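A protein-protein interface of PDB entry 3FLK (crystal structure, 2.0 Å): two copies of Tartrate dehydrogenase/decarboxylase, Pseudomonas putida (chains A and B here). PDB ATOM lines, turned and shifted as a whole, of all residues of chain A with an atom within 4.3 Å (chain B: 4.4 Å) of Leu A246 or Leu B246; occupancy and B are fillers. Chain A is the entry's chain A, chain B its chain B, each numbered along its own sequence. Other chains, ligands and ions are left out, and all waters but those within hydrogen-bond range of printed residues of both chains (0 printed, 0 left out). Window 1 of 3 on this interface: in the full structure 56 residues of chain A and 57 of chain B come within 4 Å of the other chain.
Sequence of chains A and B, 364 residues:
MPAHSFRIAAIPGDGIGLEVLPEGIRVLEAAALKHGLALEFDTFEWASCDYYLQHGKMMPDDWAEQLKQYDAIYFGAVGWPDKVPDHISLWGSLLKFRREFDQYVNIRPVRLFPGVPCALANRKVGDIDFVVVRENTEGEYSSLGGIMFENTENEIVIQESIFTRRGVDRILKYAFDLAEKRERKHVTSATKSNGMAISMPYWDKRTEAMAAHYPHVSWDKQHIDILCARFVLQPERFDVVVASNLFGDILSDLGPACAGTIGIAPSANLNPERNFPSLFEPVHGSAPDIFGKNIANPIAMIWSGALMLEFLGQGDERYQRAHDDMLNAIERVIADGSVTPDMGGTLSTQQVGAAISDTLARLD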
ATOM      1  N   GLU A 140      -4.367 -13.476   9.389  1.00  0.00           N
ATOM      2  CA  GLU A 140      -2.964 -13.759   9.076  1.00  0.00           C
ATOM      3  C   GLU A 140      -2.746 -15.132   8.445  1.00  0.00           C
ATOM      4  O   GLU A 140      -1.772 -15.334   7.720  1.00  0.00           O
ATOM      5  CB  GLU A 140      -2.088 -13.625  10.329  1.00  0.00           C
ATOM      6  CG  GLU A 140      -2.259 -12.316  11.102  1.00  0.00           C
ATOM      7  CD  GLU A 140      -3.317 -12.391  12.203  1.00  0.00           C
ATOM      8  OE1 GLU A 140      -4.266 -13.204  12.096  1.00  0.00           O
ATOM      9  OE2 GLU A 140      -3.189 -11.629  13.186  1.00  0.00           O
ATOM     10  N   TYR A 141      -3.638 -16.077   8.734  1.00  0.00           N
ATOM     11  CA  TYR A 141      -3.527 -17.409   8.156  1.00  0.00           C
ATOM     12  C   TYR A 141      -4.048 -17.403   6.734  1.00  0.00           C
ATOM     13  O   TYR A 141      -5.248 -17.273   6.483  1.00  0.00           O
ATOM     14  CB  TYR A 141      -4.205 -18.466   9.029  1.00  0.00           C
ATOM     15  CG  TYR A 141      -3.439 -18.760  10.303  1.00  0.00           C
ATOM     16  CD1 TYR A 141      -2.124 -18.315  10.471  1.00  0.00           C
ATOM     17  CD2 TYR A 141      -4.013 -19.509  11.326  1.00  0.00           C
ATOM     18  CE1 TYR A 141      -1.412 -18.589  11.634  1.00  0.00           C
ATOM     19  CE2 TYR A 141      -3.308 -19.789  12.494  1.00  0.00           C
ATOM     20  CZ  TYR A 141      -2.013 -19.327  12.641  1.00  0.00           C
ATOM     21  OH  TYR A 141      -1.314 -19.607  13.792  1.00  0.00           O
ATOM     22  N   SER A 244      -7.329 -12.056  16.624  1.00  0.00           N
ATOM     23  CA  SER A 244      -7.268 -12.527  15.240  1.00  0.00           C
ATOM     24  C   SER A 244      -6.866 -14.006  15.183  1.00  0.00           C
ATOM     25  O   SER A 244      -6.524 -14.603  16.208  1.00  0.00           O
ATOM     26  CB  SER A 244      -6.244 -11.701  14.462  1.00  0.00           C
ATOM     27  OG  SER A 244      -4.936 -11.969  14.949  1.00  0.00           O
ATOM     28  N   ASN A 245      -6.891 -14.574  13.979  1.00  0.00           N
ATOM     29  CA  ASN A 245      -6.558 -15.984  13.748  1.00  0.00           C
ATOM     30  C   ASN A 245      -5.221 -16.398  14.361  1.00  0.00           C
ATOM     31  O   ASN A 245      -5.152 -17.375  15.118  1.00  0.00           O
ATOM     32  CB  ASN A 245      -6.566 -16.285  12.244  1.00  0.00           C
ATOM     33  CG  ASN A 245      -7.132 -17.656  11.916  1.00  0.00           C
ATOM     34  OD1 ASN A 245      -7.004 -18.607  12.692  1.00  0.00           O
ATOM     35  ND2 ASN A 245      -7.760 -17.764  10.751  1.00  0.00           N
ATOM     36  N   LEU A 246      -4.170 -15.646  14.043  1.00  0.00           N
ATOM     37  CA  LEU A 246      -2.827 -15.917  14.559  1.00  0.00           C
ATOM     38  C   LEU A 246      -2.672 -15.624  16.053  1.00  0.00           C
ATOM     39  O   LEU A 246      -2.138 -16.451  16.803  1.00  0.00           O
ATOM     40  CB  LEU A 246      -1.773 -15.137  13.763  1.00  0.00           C
ATOM     41  CG  LEU A 246      -0.325 -15.164  14.281  1.00  0.00           C
ATOM     42  CD1 LEU A 246       0.260 -16.574  14.239  1.00  0.00           C
ATOM     43  CD2 LEU A 246       0.538 -14.201  13.480  1.00  0.00           C
ATOM     44  N   PHE A 247      -3.114 -14.443  16.481  1.00  0.00           N
ATOM     45  CA  PHE A 247      -2.945 -14.040  17.877  1.00  0.00           C
ATOM     46  C   PHE A 247      -3.728 -14.953  18.824  1.00  0.00           C
ATOM     47  O   PHE A 247      -3.228 -15.316  19.891  1.00  0.00           O
ATOM     48  CB  PHE A 247      -3.301 -12.559  18.092  1.00  0.00           C
ATOM     49  CG  PHE A 247      -2.352 -11.589  17.417  1.00  0.00           C
ATOM     50  CD1 PHE A 247      -1.110 -12.011  16.927  1.00  0.00           C
ATOM     51  CD2 PHE A 247      -2.689 -10.245  17.302  1.00  0.00           C
ATOM     52  CE1 PHE A 247      -0.236 -11.111  16.311  1.00  0.00           C
ATOM     53  CE2 PHE A 247      -1.821  -9.334  16.690  1.00  0.00           C
ATOM     54  CZ  PHE A 247      -0.595  -9.769  16.191  1.00  0.00           C
ATOM     55  N   GLY A 248      -4.936 -15.338  18.413  1.00  0.00           N
ATOM     56  CA  GLY A 248      -5.758 -16.291  19.159  1.00  0.00           C
ATOM     57  C   GLY A 248      -5.134 -17.674  19.246  1.00  0.00           C
ATOM     58  O   GLY A 248      -5.214 -18.335  20.283  1.00  0.00           O
ATOM     59  N   ASP A 249      -4.512 -18.108  18.153  1.00  0.00           N
ATOM     60  CA  ASP A 249      -3.756 -19.362  18.122  1.00  0.00           C
ATOM     61  C   ASP A 249      -2.652 -19.363  19.190  1.00  0.00           C
ATOM     62  O   ASP A 249      -2.561 -20.292  19.998  1.00  0.00           O
ATOM     63  CB  ASP A 249      -3.166 -19.578  16.721  1.00  0.00           C
ATOM     64  CG  ASP A 249      -2.648 -20.993  16.497  1.00  0.00           C
ATOM     65  OD1 ASP A 249      -2.537 -21.781  17.459  1.00  0.00           O
ATOM     66  OD2 ASP A 249      -2.341 -21.317  15.332  1.00  0.00           O
ATOM     67  N   ILE A 250      -1.836 -18.311  19.203  1.00  0.00           N
ATOM     68  CA  ILE A 250      -0.738 -18.178  20.167  1.00  0.00           C
ATOM     69  C   ILE A 250      -1.225 -18.165  21.623  1.00  0.00           C
ATOM     70  O   ILE A 250      -0.715 -18.914  22.466  1.00  0.00           O
ATOM     71  CB  ILE A 250       0.122 -16.922  19.880  1.00  0.00           C
ATOM     72  CG1 ILE A 250       0.842 -17.061  18.532  1.00  0.00           C
ATOM     73  CG2 ILE A 250       1.135 -16.684  21.006  1.00  0.00           C
ATOM     74  CD1 ILE A 250       1.271 -15.736  17.908  1.00  0.00           C
ATOM     75  N   GLU B 140       6.518  -9.458   8.847  1.00  0.00           N
ATOM     76  CA  GLU B 140       5.109  -9.162   9.112  1.00  0.00           C
ATOM     77  C   GLU B 140       4.836  -7.689   9.416  1.00  0.00           C
ATOM     78  O   GLU B 140       3.716  -7.216   9.225  1.00  0.00           O
ATOM     79  CB  GLU B 140       4.571 -10.032  10.255  1.00  0.00           C
ATOM     80  CG  GLU B 140       4.841 -11.532  10.105  1.00  0.00           C
ATOM     81  CD  GLU B 140       6.156 -11.975  10.738  1.00  0.00           C
ATOM     82  OE1 GLU B 140       7.092 -11.150  10.865  1.00  0.00           O
ATOM     83  OE2 GLU B 140       6.250 -13.162  11.114  1.00  0.00           O
ATOM     84  N   TYR B 141       5.845  -6.971   9.902  1.00  0.00           N
ATOM     85  CA  TYR B 141       5.670  -5.544  10.170  1.00  0.00           C
ATOM     86  C   TYR B 141       5.764  -4.761   8.870  1.00  0.00           C
ATOM     87  O   TYR B 141       6.828  -4.665   8.253  1.00  0.00           O
ATOM     88  CB  TYR B 141       6.633  -5.031  11.242  1.00  0.00           C
ATOM     89  CG  TYR B 141       6.301  -5.520  12.642  1.00  0.00           C
ATOM     90  CD1 TYR B 141       5.076  -6.136  12.920  1.00  0.00           C
ATOM     91  CD2 TYR B 141       7.195  -5.338  13.692  1.00  0.00           C
ATOM     92  CE1 TYR B 141       4.765  -6.579  14.200  1.00  0.00           C
ATOM     93  CE2 TYR B 141       6.890  -5.775  14.979  1.00  0.00           C
ATOM     94  CZ  TYR B 141       5.679  -6.395  15.222  1.00  0.00           C
ATOM     95  OH  TYR B 141       5.375  -6.828  16.493  1.00  0.00           O
ATOM     96  N   MET B 196       0.462 -20.188   8.105  1.00  0.00           N
ATOM     97  CA  MET B 196       0.997 -19.294   7.080  1.00  0.00           C
ATOM     98  C   MET B 196       1.635 -20.111   5.957  1.00  0.00           C
ATOM     99  O   MET B 196       2.803 -20.488   6.036  1.00  0.00           O
ATOM    100  CB  MET B 196       1.980 -18.297   7.697  1.00  0.00           C
ATOM    101  CG  MET B 196       1.304 -17.033   8.211  1.00  0.00           C
ATOM    102  SD  MET B 196       1.824 -16.545  10.025  1.00  0.00           S
ATOM    103  CE  MET B 196       3.669 -15.999   9.737  1.00  0.00           C
ATOM    104  N   ILE B 224       4.984 -21.279  16.552  1.00  0.00           N
ATOM    105  CA  ILE B 224       5.011 -20.166  17.498  1.00  0.00           C
ATOM    106  C   ILE B 224       4.110 -20.376  18.726  1.00  0.00           C
ATOM    107  O   ILE B 224       4.468 -19.970  19.833  1.00  0.00           O
ATOM    108  CB  ILE B 224       4.735 -18.803  16.789  1.00  0.00           C
ATOM    109  CG1 ILE B 224       4.913 -17.620  17.753  1.00  0.00           C
ATOM    110  CG2 ILE B 224       3.348 -18.784  16.143  1.00  0.00           C
ATOM    111  CD1 ILE B 224       6.333 -17.436  18.282  1.00  0.00           C
ATOM    112  N   SER B 244      11.230 -14.166  13.092  1.00  0.00           N
ATOM    113  CA  SER B 244      10.805 -13.054  12.246  1.00  0.00           C
ATOM    114  C   SER B 244      10.506 -11.800  13.080  1.00  0.00           C
ATOM    115  O   SER B 244      10.493 -11.850  14.315  1.00  0.00           O
ATOM    116  CB  SER B 244       9.560 -13.458  11.459  1.00  0.00           C
ATOM    117  OG  SER B 244       8.458 -13.629  12.341  1.00  0.00           O
ATOM    118  N   ASN B 245      10.259 -10.683  12.397  1.00  0.00           N
ATOM    119  CA  ASN B 245       9.982  -9.408  13.057  1.00  0.00           C
ATOM    120  C   ASN B 245       8.893  -9.517  14.135  1.00  0.00           C
ATOM    121  O   ASN B 245       9.103  -9.113  15.279  1.00  0.00           O
ATOM    122  CB  ASN B 245       9.605  -8.344  12.014  1.00  0.00           C
ATOM    123  CG  ASN B 245      10.156  -6.968  12.349  1.00  0.00           C
ATOM    124  OD1 ASN B 245      10.359  -6.622  13.515  1.00  0.00           O
ATOM    125  ND2 ASN B 245      10.410  -6.174  11.313  1.00  0.00           N
ATOM    126  N   LEU B 246       7.750 -10.091  13.766  1.00  0.00           N
ATOM    127  CA  LEU B 246       6.627 -10.256  14.693  1.00  0.00           C
ATOM    128  C   LEU B 246       6.892 -11.275  15.808  1.00  0.00           C
ATOM    129  O   LEU B 246       6.680 -10.975  16.988  1.00  0.00           O
ATOM    130  CB  LEU B 246       5.340 -10.617  13.936  1.00  0.00           C
ATOM    131  CG  LEU B 246       4.086 -10.973  14.750  1.00  0.00           C
ATOM    132  CD1 LEU B 246       3.589  -9.791  15.575  1.00  0.00           C
ATOM    133  CD2 LEU B 246       2.980 -11.482  13.837  1.00  0.00           C
ATOM    134  N   PHE B 247       7.349 -12.471  15.441  1.00  0.00           N
ATOM    135  CA  PHE B 247       7.529 -13.536  16.431  1.00  0.00           C
ATOM    136  C   PHE B 247       8.614 -13.174  17.445  1.00  0.00           C
ATOM    137  O   PHE B 247       8.457 -13.419  18.639  1.00  0.00           O
ATOM    138  CB  PHE B 247       7.800 -14.901  15.777  1.00  0.00           C
ATOM    139  CG  PHE B 247       6.647 -15.441  14.951  1.00  0.00           C
ATOM    140  CD1 PHE B 247       5.364 -14.897  15.048  1.00  0.00           C
ATOM    141  CD2 PHE B 247       6.847 -16.522  14.095  1.00  0.00           C
ATOM    142  CE1 PHE B 247       4.309 -15.404  14.285  1.00  0.00           C
ATOM    143  CE2 PHE B 247       5.796 -17.042  13.329  1.00  0.00           C
ATOM    144  CZ  PHE B 247       4.526 -16.481  13.424  1.00  0.00           C
ATOM    145  N   GLY B 248       9.692 -12.555  16.964  1.00  0.00           N
ATOM    146  CA  GLY B 248      10.771 -12.078  17.827  1.00  0.00           C
ATOM    147  C   GLY B 248      10.302 -11.026  18.816  1.00  0.00           C
ATOM    148  O   GLY B 248      10.735 -11.006  19.968  1.00  0.00           O
ATOM    149  N   ASP B 249       9.411 -10.150  18.360  1.00  0.00           N
ATOM    150  CA  ASP B 249       8.807  -9.129  19.212  1.00  0.00           C
ATOM    151  C   ASP B 249       8.050  -9.774  20.381  1.00  0.00           C
ATOM    152  O   ASP B 249       8.292  -9.442  21.545  1.00  0.00           O
ATOM    153  CB  ASP B 249       7.866  -8.256  18.377  1.00  0.00           C
ATOM    154  CG  ASP B 249       7.389  -7.010  19.115  1.00  0.00           C
ATOM    155  OD1 ASP B 249       7.693  -6.829  20.312  1.00  0.00           O
ATOM    156  OD2 ASP B 249       6.703  -6.192  18.475  1.00  0.00           O
ATOM    157  N   ILE B 250       7.149 -10.701  20.057  1.00  0.00           N
ATOM    158  CA  ILE B 250       6.357 -11.424  21.054  1.00  0.00           C
ATOM    159  C   ILE B 250       7.250 -12.160  22.058  1.00  0.00           C
ATOM    160  O   ILE B 250       7.088 -12.010  23.269  1.00  0.00           O
ATOM    161  CB  ILE B 250       5.371 -12.419  20.386  1.00  0.00           C
ATOM    162  CG1 ILE B 250       4.326 -11.658  19.561  1.00  0.00           C
ATOM    163  CG2 ILE B 250       4.692 -13.308  21.437  1.00  0.00           C
ATOM    164  CD1 ILE B 250       3.532 -12.525  18.593  1.00  0.00           C
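Of chain B, only Leu B246 comes within 4 Å of Leu A246.
Of the printed residues of chain B, Tyr A141 touches Met B196 (3.97 Å).
Of the printed residues of chain A, Ile B250 touches Ile A250.
Of the printed residues of chain A, Met B196 touches Glu A140 and Tyr A141.
Of the printed residues of chain A, Ile B224 touches Ile A250 (3.9 Å).
The nearest residue of chain B that does not touch Leu A246 is Phe B247 (4.04 Å).
Leu A246 touches its own counterpart, Leu B246.
Ile B250 touches its own counterpart, Ile A250.
Positions printed for both chains: 140, 141, 244, 245, 246, 247, 248, 249 and 250.
Of the 5 pairs that touch across the chains among the printed residues, 2 have their exchanged pair printed and touching as well.
Hydrophobic or aromatic side chains of chain B within 4 Å of the printed part of chain A: Met B196, Ile B224, Leu B246 and Ile B250.
Among the printed residues, 5 pairs touch across the chains.
Among the printed residues, no Asp or Glu carboxylate lies within 4 Å of a Lys or Arg side-chain nitrogen of the other chain.
The side-chain hydroxyl of Ser A244 sits at hydrogen-bond distance from the side-chain carboxylate of Glu A140 (2.5 Å).
The side-chain carboxylate of Glu A140 is in hydrogen-bond range of the backbone NH of Leu A246 (3.1 Å).
OH of Tyr A141 is in hydrogen-bond range of OD2 of Asp A249 (2.5 Å).
The backbone NH (N) of Leu B246 lies within hydrogen-bond range of the side-chain carboxylate (OE1) of Glu B140.
Among the printed residues, merely in contact across the chains: Glu A140 with Met B196 (3.5 Å), Leu A246 with Leu B246 (3.7 Å), Ile A250 with Ile B224 (3.9 Å), Tyr A141 with Met B196 (3.97 Å) and Ile A250 with Ile B250 (3.99 Å).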
